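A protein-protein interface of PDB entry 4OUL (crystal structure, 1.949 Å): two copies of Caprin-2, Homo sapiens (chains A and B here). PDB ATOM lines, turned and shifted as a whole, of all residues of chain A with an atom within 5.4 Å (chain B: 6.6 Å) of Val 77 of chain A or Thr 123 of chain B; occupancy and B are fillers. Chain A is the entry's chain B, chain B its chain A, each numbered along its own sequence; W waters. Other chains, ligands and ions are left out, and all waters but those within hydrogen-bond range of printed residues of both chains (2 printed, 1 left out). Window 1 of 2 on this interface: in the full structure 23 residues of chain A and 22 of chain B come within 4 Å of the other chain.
The side-chain amide oxygen (OD1) of Asn 93 of chain A sits at hydrogen-bond distance from a ring nitrogen (ND1) of His 55 of chain B, at 3.5 Å.
ND1 of His 55 of chain B is in hydrogen-bond range of ND1 of His 94 of chain A, 3.0 Å away.
The backbone carbonyl oxygen of Trp 119 of chain B lies within hydrogen-bond range of the side-chain hydroxyl of Ser 78 of chain A (2.8 Å).
NZ of Lys 120 of chain B is in hydrogen-bond range of O of Val 75 of chain A, 3.1 Å away.
The side-chain amino group of Lys 120 of chain B is in hydrogen-bond range of the backbone carbonyl oxygen of Leu 76 of chain A (2.8 Å).
O of Lys 120 of chain B is in hydrogen-bond range of N of Ser 78 of chain A (3.0 Å).
The backbone carbonyl oxygen of Tyr 121 of chain B sits at hydrogen-bond distance from the side-chain amide nitrogen of Asn 93 of chain A (3.1 Å).
The side-chain amide oxygen (OD1) of Asn 93 of chain A sits at hydrogen-bond distance from the side-chain hydroxyl (OG1) of Thr 123 of chain B, at 2.7 Å.
The side-chain hydroxyl (OG1) of Thr 123 of chain B sits close to a ring nitrogen (ND1) of His 94 of chain A, 3.4 Å away.
The side-chain hydroxyl (OG) of Ser 125 of chain B lies within hydrogen-bond range of a ring nitrogen (NE2) of His 94 of chain A, at 2.5 Å.
The backbone carbonyl oxygen (O) of Ser 6 of chain B sits at hydrogen-bond distance from the backbone NH (N) of Leu 28 of chain B, 2.5 Å away.
OG of Ser 6 of chain B lies within hydrogen-bond range of OG of Ser 125 of chain B.
O of Ile 53 of chain B lies within hydrogen-bond range of N of Ser 125 of chain B, at 3.0 Å.
The backbone carbonyl oxygen of Leu 69 of chain A sits at hydrogen-bond distance from the backbone NH of Leu 76 of chain A, 2.8 Å away.
The backbone NH of Leu 69 of chain A is in hydrogen-bond range of the backbone carbonyl oxygen of Val 77 of chain A, at 2.8 Å.
The side-chain amide nitrogen (ND2) of Asn 93 of chain A is in hydrogen-bond range of the backbone carbonyl oxygen (O) of Ser 78 of chain A (2.7 Å).
Asn 68 of chain A touches Trp 119 of chain B (ND2 to CE3, 3.4 Å).
Val 75 of chain A touches Trp 119 of chain B (CG2 to NE1, 3.9 Å).
CD1 of Leu 28 of chain B touches CG1 of Val 77 of chain A, at 3.7 Å.
Lys 120 of chain B touches Val 77 of chain A.
CG1 of Val 77 of chain A touches CG2 of Thr 123 of chain B, 3.8 Å away.
CA of Tyr 121 of chain B touches O of Ser 78 of chain A, 3.5 Å away.
Ala 79 of chain A touches Tyr 121 of chain B.
Asn 93 of chain A touches Lys 120 of chain B (ND2 to O, 3.6 Å).
His 94 of chain A touches Ile 53 of chain B.
His 94 of chain A touches Phe 124 of chain B.
Printed residues of chain B within 4 Å of Leu 76 of chain A: Lys 120.
Val 77 of chain A touches four residues of chain B.
Printed residues of chain B within 4 Å of Ala 79 of chain A: Tyr 121 (3.8 Å).
Ala 7 of chain B touches none of the printed residues of chain A.
Of the printed residues of chain A, Leu 28 of chain B touches Val 77 (3.7 Å).
Printed residues of chain A within 4 Å of Ile 53 of chain B: His 94 (3.4 Å).
Leu 57 of chain B touches none of the printed residues of chain A.
Of the printed residues of chain A, Trp 119 of chain B touches Asn 68, Val 75, Val 77 and Ser 78.
Thr 123 of chain B touches just these residues of chain A: Val 77, Asn 93 and His 94.
The nearest residue of chain B that does not touch Val 77 of chain A is Tyr 121 of chain B (5.5 Å).
The nearest printed residue of chain A that does not touch Thr 123 of chain B is Ser 78 of chain A (6.1 Å).
The nearest printed residue of chain B that does not touch Asn 93 of chain A is Ser 122 of chain B (4.8 Å).
Of the 12 printed residues of chain A, 8 touch a printed residue of chain B.
Hydrophobic or aromatic side chains of chain A within 4 Å of the printed part of chain B: Val 75, Val 77 and His 94.
Hydrophobic or aromatic side chains of chain B that line the printed part of chain A: Leu 28, Ile 53, His 55, Trp 119 and Tyr 121.
Along chain B the printed residues that touch a printed residue of chain A span positions 28 to 125.
Position printed for both chains: 54.
Water W1 bridges the backbone carbonyl oxygen of Val 75 of chain A (2.8 Å) and the side-chain amino group of Lys 120 of chain B (3.5 Å).
Water W2 lies within hydrogen-bond range of the backbone carbonyl oxygen (O) of Tyr 121 of chain B and the side-chain amide nitrogen (ND2) of Asn 93 of chain A.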
ATOM      1  N   PHE A  54     -16.624  12.856  21.116  1.00  0.00           N
ATOM      2  CA  PHE A  54     -16.531  11.730  20.222  1.00  0.00           C
ATOM      3  C   PHE A  54     -16.311  10.448  21.034  1.00  0.00           C
ATOM      4  O   PHE A  54     -15.710  10.474  22.110  1.00  0.00           O
ATOM      5  CB  PHE A  54     -15.411  11.961  19.186  1.00  0.00           C
ATOM      6  CG  PHE A  54     -14.014  11.961  19.775  1.00  0.00           C
ATOM      7  CD1 PHE A  54     -13.281  10.780  19.862  1.00  0.00           C
ATOM      8  CD2 PHE A  54     -13.423  13.136  20.206  1.00  0.00           C
ATOM      9  CE1 PHE A  54     -11.996  10.766  20.394  1.00  0.00           C
ATOM     10  CE2 PHE A  54     -12.130  13.123  20.741  1.00  0.00           C
ATOM     11  CZ  PHE A  54     -11.423  11.948  20.826  1.00  0.00           C
ATOM     12  N   VAL A  67      -6.685   8.353  18.738  1.00  0.00           N
ATOM     13  CA  VAL A  67      -7.501   9.309  17.984  1.00  0.00           C
ATOM     14  C   VAL A  67      -7.167  10.726  18.433  1.00  0.00           C
ATOM     15  O   VAL A  67      -7.032  10.970  19.621  1.00  0.00           O
ATOM     16  CB  VAL A  67      -8.994   9.026  18.187  1.00  0.00           C
ATOM     17  CG1 VAL A  67      -9.876  10.096  17.479  1.00  0.00           C
ATOM     18  CG2 VAL A  67      -9.328   7.599  17.733  1.00  0.00           C
ATOM     19  N   ASN A  68      -7.007  11.655  17.494  1.00  0.00           N
ATOM     20  CA  ASN A  68      -6.830  13.057  17.863  1.00  0.00           C
ATOM     21  C   ASN A  68      -8.026  13.879  17.401  1.00  0.00           C
ATOM     22  O   ASN A  68      -8.515  13.724  16.277  1.00  0.00           O
ATOM     23  CB  ASN A  68      -5.576  13.678  17.243  1.00  0.00           C
ATOM     24  CG  ASN A  68      -4.355  12.802  17.359  1.00  0.00           C
ATOM     25  OD1 ASN A  68      -3.823  12.343  16.338  1.00  0.00           O
ATOM     26  ND2 ASN A  68      -3.868  12.604  18.573  1.00  0.00           N
ATOM     27  N   LEU A  69      -8.493  14.769  18.260  1.00  0.00           N
ATOM     28  CA  LEU A  69      -9.390  15.806  17.783  1.00  0.00           C
ATOM     29  C   LEU A  69      -8.492  16.899  17.223  1.00  0.00           C
ATOM     30  O   LEU A  69      -7.611  17.403  17.919  1.00  0.00           O
ATOM     31  CB  LEU A  69     -10.282  16.352  18.894  1.00  0.00           C
ATOM     32  CG  LEU A  69     -11.218  17.488  18.450  1.00  0.00           C
ATOM     33  CD1 LEU A  69     -12.353  16.953  17.611  1.00  0.00           C
ATOM     34  CD2 LEU A  69     -11.742  18.302  19.641  1.00  0.00           C
ATOM     35  N   VAL A  75      -3.267  19.357  17.065  1.00  0.00           N
ATOM     36  CA  VAL A  75      -3.916  18.443  18.003  1.00  0.00           C
ATOM     37  C   VAL A  75      -4.541  19.197  19.175  1.00  0.00           C
ATOM     38  O   VAL A  75      -3.846  19.885  19.909  1.00  0.00           O
ATOM     39  CB  VAL A  75      -2.929  17.396  18.558  1.00  0.00           C
ATOM     40  CG1 VAL A  75      -3.606  16.547  19.641  1.00  0.00           C
ATOM     41  CG2 VAL A  75      -2.391  16.532  17.425  1.00  0.00           C
ATOM     42  N   LEU A  76      -5.851  19.065  19.346  1.00  0.00           N
ATOM     43  CA  LEU A  76      -6.553  19.710  20.447  1.00  0.00           C
ATOM     44  C   LEU A  76      -6.540  18.816  21.679  1.00  0.00           C
ATOM     45  O   LEU A  76      -5.984  19.177  22.721  1.00  0.00           O
ATOM     46  CB  LEU A  76      -7.994  20.016  20.055  1.00  0.00           C
ATOM     47  CG  LEU A  76      -8.214  21.066  18.968  1.00  0.00           C
ATOM     48  CD1 LEU A  76      -9.670  21.086  18.530  1.00  0.00           C
ATOM     49  CD2 LEU A  76      -7.777  22.437  19.434  1.00  0.00           C
ATOM     50  N   VAL A  77      -7.221  17.677  21.572  1.00  0.00           N
ATOM     51  CA  VAL A  77      -7.218  16.662  22.622  1.00  0.00           C
ATOM     52  C   VAL A  77      -7.101  15.283  21.977  1.00  0.00           C
ATOM     53  O   VAL A  77      -7.401  15.128  20.787  1.00  0.00           O
ATOM     54  CB  VAL A  77      -8.492  16.707  23.493  1.00  0.00           C
ATOM     55  CG1 VAL A  77      -8.635  18.092  24.198  1.00  0.00           C
ATOM     56  CG2 VAL A  77      -9.729  16.341  22.656  1.00  0.00           C
ATOM     57  N   SER A  78      -6.729  14.275  22.760  1.00  0.00           N
ATOM     58  CA  SER A  78      -6.560  12.941  22.187  1.00  0.00           C
ATOM     59  C   SER A  78      -7.272  11.869  23.004  1.00  0.00           C
ATOM     60  O   SER A  78      -7.688  12.113  24.127  1.00  0.00           O
ATOM     61  CB  SER A  78      -5.072  12.614  22.059  1.00  0.00           C
ATOM     62  OG  SER A  78      -4.439  13.549  21.203  1.00  0.00           O
ATOM     63  N   ALA A  79      -7.463  10.689  22.418  1.00  0.00           N
ATOM     64  CA  ALA A  79      -8.059   9.577  23.158  1.00  0.00           C
ATOM     65  C   ALA A  79      -7.296   8.311  22.839  1.00  0.00           C
ATOM     66  O   ALA A  79      -6.722   8.197  21.765  1.00  0.00           O
ATOM     67  CB  ALA A  79      -9.546   9.405  22.822  1.00  0.00           C
ATOM     68  N   ASN A  93     -13.232  11.434  23.990  1.00  0.00           N
ATOM     69  CA  ASN A  93     -12.858  12.678  24.632  1.00  0.00           C
ATOM     70  C   ASN A  93     -13.805  13.820  24.215  1.00  0.00           C
ATOM     71  O   ASN A  93     -14.743  13.611  23.462  1.00  0.00           O
ATOM     72  CB  ASN A  93     -11.411  13.063  24.324  1.00  0.00           C
ATOM     73  CG  ASN A  93     -10.757  13.772  25.476  1.00  0.00           C
ATOM     74  OD1 ASN A  93     -11.427  14.455  26.266  1.00  0.00           O
ATOM     75  ND2 ASN A  93      -9.440  13.641  25.575  1.00  0.00           N
ATOM     76  N   HIS A  94     -13.535  15.021  24.714  1.00  0.00           N
ATOM     77  CA  HIS A  94     -14.408  16.171  24.459  1.00  0.00           C
ATOM     78  C   HIS A  94     -13.542  17.415  24.453  1.00  0.00           C
ATOM     79  O   HIS A  94     -12.401  17.377  24.920  1.00  0.00           O
ATOM     80  CB  HIS A  94     -15.449  16.318  25.558  1.00  0.00           C
ATOM     81  CG  HIS A  94     -14.864  16.876  26.811  1.00  0.00           C
ATOM     82  ND1 HIS A  94     -14.171  16.102  27.717  1.00  0.00           N
ATOM     83  CD2 HIS A  94     -14.773  18.151  27.260  1.00  0.00           C
ATOM     84  CE1 HIS A  94     -13.719  16.868  28.694  1.00  0.00           C
ATOM     85  NE2 HIS A  94     -14.062  18.119  28.433  1.00  0.00           N
ATOM     86  N   ALA A  95     -14.089  18.531  23.971  1.00  0.00           N
ATOM     87  CA  ALA A  95     -13.382  19.784  24.069  1.00  0.00           C
ATOM     88  C   ALA A  95     -14.382  20.933  23.956  1.00  0.00           C
ATOM     89  O   ALA A  95     -15.435  20.777  23.342  1.00  0.00           O
ATOM     90  CB  ALA A  95     -12.319  19.885  22.982  1.00  0.00           C
ATOM     91  N   SER B   6     -12.375  24.664  29.719  1.00  0.00           N
ATOM     92  CA  SER B   6     -11.911  23.377  29.238  1.00  0.00           C
ATOM     93  C   SER B   6     -10.468  23.298  29.677  1.00  0.00           C
ATOM     94  O   SER B   6      -9.674  24.168  29.332  1.00  0.00           O
ATOM     95  CB  SER B   6     -12.072  23.274  27.716  1.00  0.00           C
ATOM     96  OG  SER B   6     -11.941  21.943  27.269  1.00  0.00           O
ATOM     97  N   ALA B   7     -10.135  22.304  30.501  1.00  0.00           N
ATOM     98  CA  ALA B   7      -8.783  22.182  31.034  1.00  0.00           C
ATOM     99  C   ALA B   7      -8.195  20.840  30.660  1.00  0.00           C
ATOM    100  O   ALA B   7      -8.938  19.879  30.455  1.00  0.00           O
ATOM    101  CB  ALA B   7      -8.764  22.334  32.570  1.00  0.00           C
ATOM    102  N   ALA B   8      -6.867  20.792  30.581  1.00  0.00           N
ATOM    103  CA  ALA B   8      -6.144  19.562  30.263  1.00  0.00           C
ATOM    104  C   ALA B   8      -4.881  19.437  31.105  1.00  0.00           C
ATOM    105  O   ALA B   8      -4.317  20.447  31.555  1.00  0.00           O
ATOM    106  CB  ALA B   8      -5.796  19.511  28.788  1.00  0.00           C
ATOM    107  N   ARG B   9      -4.439  18.193  31.299  1.00  0.00           N
ATOM    108  CA  ARG B   9      -3.181  17.876  31.963  1.00  0.00           C
ATOM    109  C   ARG B   9      -2.134  17.456  30.928  1.00  0.00           C
ATOM    110  O   ARG B   9      -2.400  16.576  30.112  1.00  0.00           O
ATOM    111  CB  ARG B   9      -3.381  16.755  32.993  1.00  0.00           C
ATOM    112  CG  ARG B   9      -3.732  17.250  34.388  1.00  0.00           C
ATOM    113  CD  ARG B   9      -3.062  16.430  35.486  1.00  0.00           C
ATOM    114  NE  ARG B   9      -1.604  16.538  35.496  1.00  0.00           N
ATOM    115  CZ  ARG B   9      -0.928  17.485  36.143  1.00  0.00           C
ATOM    116  NH1 ARG B   9      -1.576  18.414  36.849  1.00  0.00           N
ATOM    117  NH2 ARG B   9       0.400  17.497  36.096  1.00  0.00           N
ATOM    118  N   PHE B  24      -4.755  21.242  36.946  1.00  0.00           N
ATOM    119  CA  PHE B  24      -4.455  21.266  35.518  1.00  0.00           C
ATOM    120  C   PHE B  24      -3.381  22.286  35.175  1.00  0.00           C
ATOM    121  O   PHE B  24      -3.118  23.193  35.954  1.00  0.00           O
ATOM    122  CB  PHE B  24      -5.743  21.542  34.742  1.00  0.00           C
ATOM    123  CG  PHE B  24      -6.754  20.464  34.907  1.00  0.00           C
ATOM    124  CD1 PHE B  24      -7.580  20.447  36.016  1.00  0.00           C
ATOM    125  CD2 PHE B  24      -6.850  19.438  33.980  1.00  0.00           C
ATOM    126  CE1 PHE B  24      -8.497  19.438  36.201  1.00  0.00           C
ATOM    127  CE2 PHE B  24      -7.776  18.427  34.151  1.00  0.00           C
ATOM    128  CZ  PHE B  24      -8.599  18.426  35.277  1.00  0.00           C
ATOM    129  N   LEU B  28      -7.927  25.275  27.858  1.00  0.00           N
ATOM    130  CA  LEU B  28      -8.246  25.315  26.438  1.00  0.00           C
ATOM    131  C   LEU B  28      -9.273  26.420  26.182  1.00  0.00           C
ATOM    132  O   LEU B  28      -9.480  26.830  25.041  1.00  0.00           O
ATOM    133  CB  LEU B  28      -8.778  23.958  25.961  1.00  0.00           C
ATOM    134  CG  LEU B  28      -7.753  22.812  26.026  1.00  0.00           C
ATOM    135  CD1 LEU B  28      -8.384  21.415  25.897  1.00  0.00           C
ATOM    136  CD2 LEU B  28      -6.679  23.010  24.966  1.00  0.00           C
ATOM    137  N   ILE B  53     -18.128  17.618  32.126  1.00  0.00           N
ATOM    138  CA  ILE B  53     -17.690  16.375  31.516  1.00  0.00           C
ATOM    139  C   ILE B  53     -16.207  16.204  31.771  1.00  0.00           C
ATOM    140  O   ILE B  53     -15.461  17.179  31.813  1.00  0.00           O
ATOM    141  CB  ILE B  53     -18.009  16.346  29.996  1.00  0.00           C
ATOM    142  CG1 ILE B  53     -17.537  15.029  29.357  1.00  0.00           C
ATOM    143  CG2 ILE B  53     -17.364  17.517  29.300  1.00  0.00           C
ATOM    144  CD1 ILE B  53     -18.097  14.803  27.970  1.00  0.00           C
ATOM    145  N   PHE B  54     -15.764  14.961  31.966  1.00  0.00           N
ATOM    146  CA  PHE B  54     -14.352  14.763  32.133  1.00  0.00           C
ATOM    147  C   PHE B  54     -13.894  13.411  31.568  1.00  0.00           C
ATOM    148  O   PHE B  54     -14.676  12.473  31.444  1.00  0.00           O
ATOM    149  CB  PHE B  54     -13.963  14.914  33.613  1.00  0.00           C
ATOM    150  CG  PHE B  54     -14.506  13.827  34.511  1.00  0.00           C
ATOM    151  CD1 PHE B  54     -13.777  12.663  34.717  1.00  0.00           C
ATOM    152  CD2 PHE B  54     -15.696  13.997  35.197  1.00  0.00           C
ATOM    153  CE1 PHE B  54     -14.244  11.678  35.558  1.00  0.00           C
ATOM    154  CE2 PHE B  54     -16.164  12.999  36.046  1.00  0.00           C
ATOM    155  CZ  PHE B  54     -15.436  11.842  36.213  1.00  0.00           C
ATOM    156  N   HIS B  55     -12.642  13.387  31.135  1.00  0.00           N
ATOM    157  CA  HIS B  55     -11.964  12.171  30.670  1.00  0.00           C
ATOM    158  C   HIS B  55     -10.576  12.128  31.307  1.00  0.00           C
ATOM    159  O   HIS B  55      -9.792  13.047  31.107  1.00  0.00           O
ATOM    160  CB  HIS B  55     -11.848  12.160  29.145  1.00  0.00           C
ATOM    161  CG  HIS B  55     -13.159  12.050  28.442  1.00  0.00           C
ATOM    162  ND1 HIS B  55     -13.979  13.139  28.208  1.00  0.00           N
ATOM    163  CD2 HIS B  55     -13.812  10.974  27.935  1.00  0.00           C
ATOM    164  CE1 HIS B  55     -15.059  12.740  27.564  1.00  0.00           C
ATOM    165  NE2 HIS B  55     -14.991  11.434  27.397  1.00  0.00           N
ATOM    166  N   MET B  56     -10.274  11.077  32.065  1.00  0.00           N
ATOM    167  CA  MET B  56      -8.960  10.941  32.708  1.00  0.00           C
ATOM    168  C   MET B  56      -8.321   9.637  32.234  1.00  0.00           C
ATOM    169  O   MET B  56      -8.874   8.564  32.423  1.00  0.00           O
ATOM    170  CB  MET B  56      -9.074  10.960  34.250  1.00  0.00           C
ATOM    171  CG  MET B  56      -9.592  12.315  34.827  1.00  0.00           C
ATOM    172  SD  MET B  56      -8.362  13.629  34.683  1.00  0.00           S
ATOM    173  CE  MET B  56      -9.327  14.944  33.906  1.00  0.00           C
ATOM    174  N   LEU B  57      -7.161   9.743  31.611  1.00  0.00           N
ATOM    175  CA  LEU B  57      -6.432   8.566  31.207  1.00  0.00           C
ATOM    176  C   LEU B  57      -5.535   8.187  32.366  1.00  0.00           C
ATOM    177  O   LEU B  57      -4.806   9.037  32.884  1.00  0.00           O
ATOM    178  CB  LEU B  57      -5.604   8.833  29.947  1.00  0.00           C
ATOM    179  CG  LEU B  57      -4.997   7.613  29.246  1.00  0.00           C
ATOM    180  CD1 LEU B  57      -6.076   6.833  28.491  1.00  0.00           C
ATOM    181  CD2 LEU B  57      -3.862   8.018  28.316  1.00  0.00           C
ATOM    182  N   LEU B 107     -12.470  18.135  40.372  1.00  0.00           N
ATOM    183  CA  LEU B 107     -12.211  16.710  40.229  1.00  0.00           C
ATOM    184  C   LEU B 107     -11.273  16.192  41.311  1.00  0.00           C
ATOM    185  O   LEU B 107     -10.193  16.743  41.552  1.00  0.00           O
ATOM    186  CB  LEU B 107     -11.613  16.407  38.861  1.00  0.00           C
ATOM    187  CG  LEU B 107     -12.536  16.529  37.655  1.00  0.00           C
ATOM    188  CD1 LEU B 107     -11.775  16.029  36.435  1.00  0.00           C
ATOM    189  CD2 LEU B 107     -13.818  15.740  37.870  1.00  0.00           C
ATOM    190  N   TRP B 119      -0.341  15.677  24.040  1.00  0.00           N
ATOM    191  CA  TRP B 119      -1.499  15.242  23.257  1.00  0.00           C
ATOM    192  C   TRP B 119      -2.836  15.324  24.014  1.00  0.00           C
ATOM    193  O   TRP B 119      -3.909  15.176  23.418  1.00  0.00           O
ATOM    194  CB  TRP B 119      -1.249  13.833  22.706  1.00  0.00           C
ATOM    195  CG  TRP B 119      -0.662  13.870  21.323  1.00  0.00           C
ATOM    196  CD1 TRP B 119      -0.029  14.925  20.730  1.00  0.00           C
ATOM    197  CD2 TRP B 119      -0.681  12.817  20.353  1.00  0.00           C
ATOM    198  NE1 TRP B 119       0.342  14.592  19.439  1.00  0.00           N
ATOM    199  CE2 TRP B 119      -0.044  13.302  19.192  1.00  0.00           C
ATOM    200  CE3 TRP B 119      -1.183  11.519  20.353  1.00  0.00           C
ATOM    201  CZ2 TRP B 119       0.108  12.527  18.045  1.00  0.00           C
ATOM    202  CZ3 TRP B 119      -1.036  10.751  19.216  1.00  0.00           C
ATOM    203  CH2 TRP B 119      -0.390  11.254  18.079  1.00  0.00           C
ATOM    204  N   LYS B 120      -2.763  15.590  25.314  1.00  0.00           N
ATOM    205  CA  LYS B 120      -3.932  15.948  26.110  1.00  0.00           C
ATOM    206  C   LYS B 120      -5.036  14.914  26.115  1.00  0.00           C
ATOM    207  O   LYS B 120      -6.114  15.123  25.539  1.00  0.00           O
ATOM    208  CB  LYS B 120      -4.529  17.275  25.625  1.00  0.00           C
ATOM    209  CG  LYS B 120      -3.561  18.432  25.626  1.00  0.00           C
ATOM    210  CD  LYS B 120      -4.283  19.700  25.229  1.00  0.00           C
ATOM    211  CE  LYS B 120      -3.424  20.546  24.348  1.00  0.00           C
ATOM    212  NZ  LYS B 120      -3.312  20.005  22.967  1.00  0.00           N
ATOM    213  N   TYR B 121      -4.776  13.808  26.782  1.00  0.00           N
ATOM    214  CA  TYR B 121      -5.774  12.760  26.928  1.00  0.00           C
ATOM    215  C   TYR B 121      -6.726  13.085  28.102  1.00  0.00           C
ATOM    216  O   TYR B 121      -7.875  12.657  28.113  1.00  0.00           O
ATOM    217  CB  TYR B 121      -5.084  11.401  27.136  1.00  0.00           C
ATOM    218  CG  TYR B 121      -4.199  10.947  25.972  1.00  0.00           C
ATOM    219  CD1 TYR B 121      -2.844  11.290  25.917  1.00  0.00           C
ATOM    220  CD2 TYR B 121      -4.719  10.178  24.932  1.00  0.00           C
ATOM    221  CE1 TYR B 121      -2.033  10.879  24.846  1.00  0.00           C
ATOM    222  CE2 TYR B 121      -3.923   9.772  23.866  1.00  0.00           C
ATOM    223  CZ  TYR B 121      -2.588  10.122  23.831  1.00  0.00           C
ATOM    224  OH  TYR B 121      -1.822   9.714  22.762  1.00  0.00           O
ATOM    225  N   SER B 122      -6.243  13.846  29.083  1.00  0.00           N
ATOM    226  CA  SER B 122      -6.960  14.038  30.343  1.00  0.00           C
ATOM    227  C   SER B 122      -7.507  15.452  30.464  1.00  0.00           C
ATOM    228  O   SER B 122      -6.744  16.411  30.613  1.00  0.00           O
ATOM    229  CB  SER B 122      -6.067  13.737  31.550  1.00  0.00           C
ATOM    230  OG  SER B 122      -5.620  12.389  31.520  1.00  0.00           O
ATOM    231  N   THR B 123      -8.834  15.531  30.430  1.00  0.00           N
ATOM    232  CA  THR B 123      -9.579  16.767  30.216  1.00  0.00           C
ATOM    233  C   THR B 123     -10.765  16.918  31.158  1.00  0.00           C
ATOM    234  O   THR B 123     -11.325  15.934  31.639  1.00  0.00           O
ATOM    235  CB  THR B 123     -10.134  16.823  28.792  1.00  0.00           C
ATOM    236  OG1 THR B 123     -10.915  15.640  28.599  1.00  0.00           O
ATOM    237  CG2 THR B 123      -9.002  16.875  27.750  1.00  0.00           C
ATOM    238  N   PHE B 124     -11.160  18.169  31.378  1.00  0.00           N
ATOM    239  CA  PHE B 124     -12.255  18.534  32.282  1.00  0.00           C
ATOM    240  C   PHE B 124     -12.830  19.843  31.771  1.00  0.00           C
ATOM    241  O   PHE B 124     -12.091  20.821  31.700  1.00  0.00           O
ATOM    242  CB  PHE B 124     -11.721  18.700  33.700  1.00  0.00           C
ATOM    243  CG  PHE B 124     -12.748  19.129  34.734  1.00  0.00           C
ATOM    244  CD1 PHE B 124     -14.075  18.739  34.651  1.00  0.00           C
ATOM    245  CD2 PHE B 124     -12.345  19.930  35.811  1.00  0.00           C
ATOM    246  CE1 PHE B 124     -15.001  19.150  35.618  1.00  0.00           C
ATOM    247  CE2 PHE B 124     -13.265  20.350  36.790  1.00  0.00           C
ATOM    248  CZ  PHE B 124     -14.588  19.954  36.696  1.00  0.00           C
ATOM    249  N   SER B 125     -14.116  19.850  31.428  1.00  0.00           N
ATOM    250  CA  SER B 125     -14.794  21.046  30.913  1.00  0.00           C
ATOM    251  C   SER B 125     -16.131  21.267  31.593  1.00  0.00           C
ATOM    252  O   SER B 125     -16.707  20.353  32.185  1.00  0.00           O
ATOM    253  CB  SER B 125     -15.039  20.936  29.412  1.00  0.00           C
ATOM    254  OG  SER B 125     -13.845  20.632  28.716  1.00  0.00           O
HETATM  255  O   HOH W   1      -1.126  20.558  20.298  1.00  0.00           O
HETATM  256  O   HOH W   2      -9.414  10.523  26.893  1.00  0.00           O
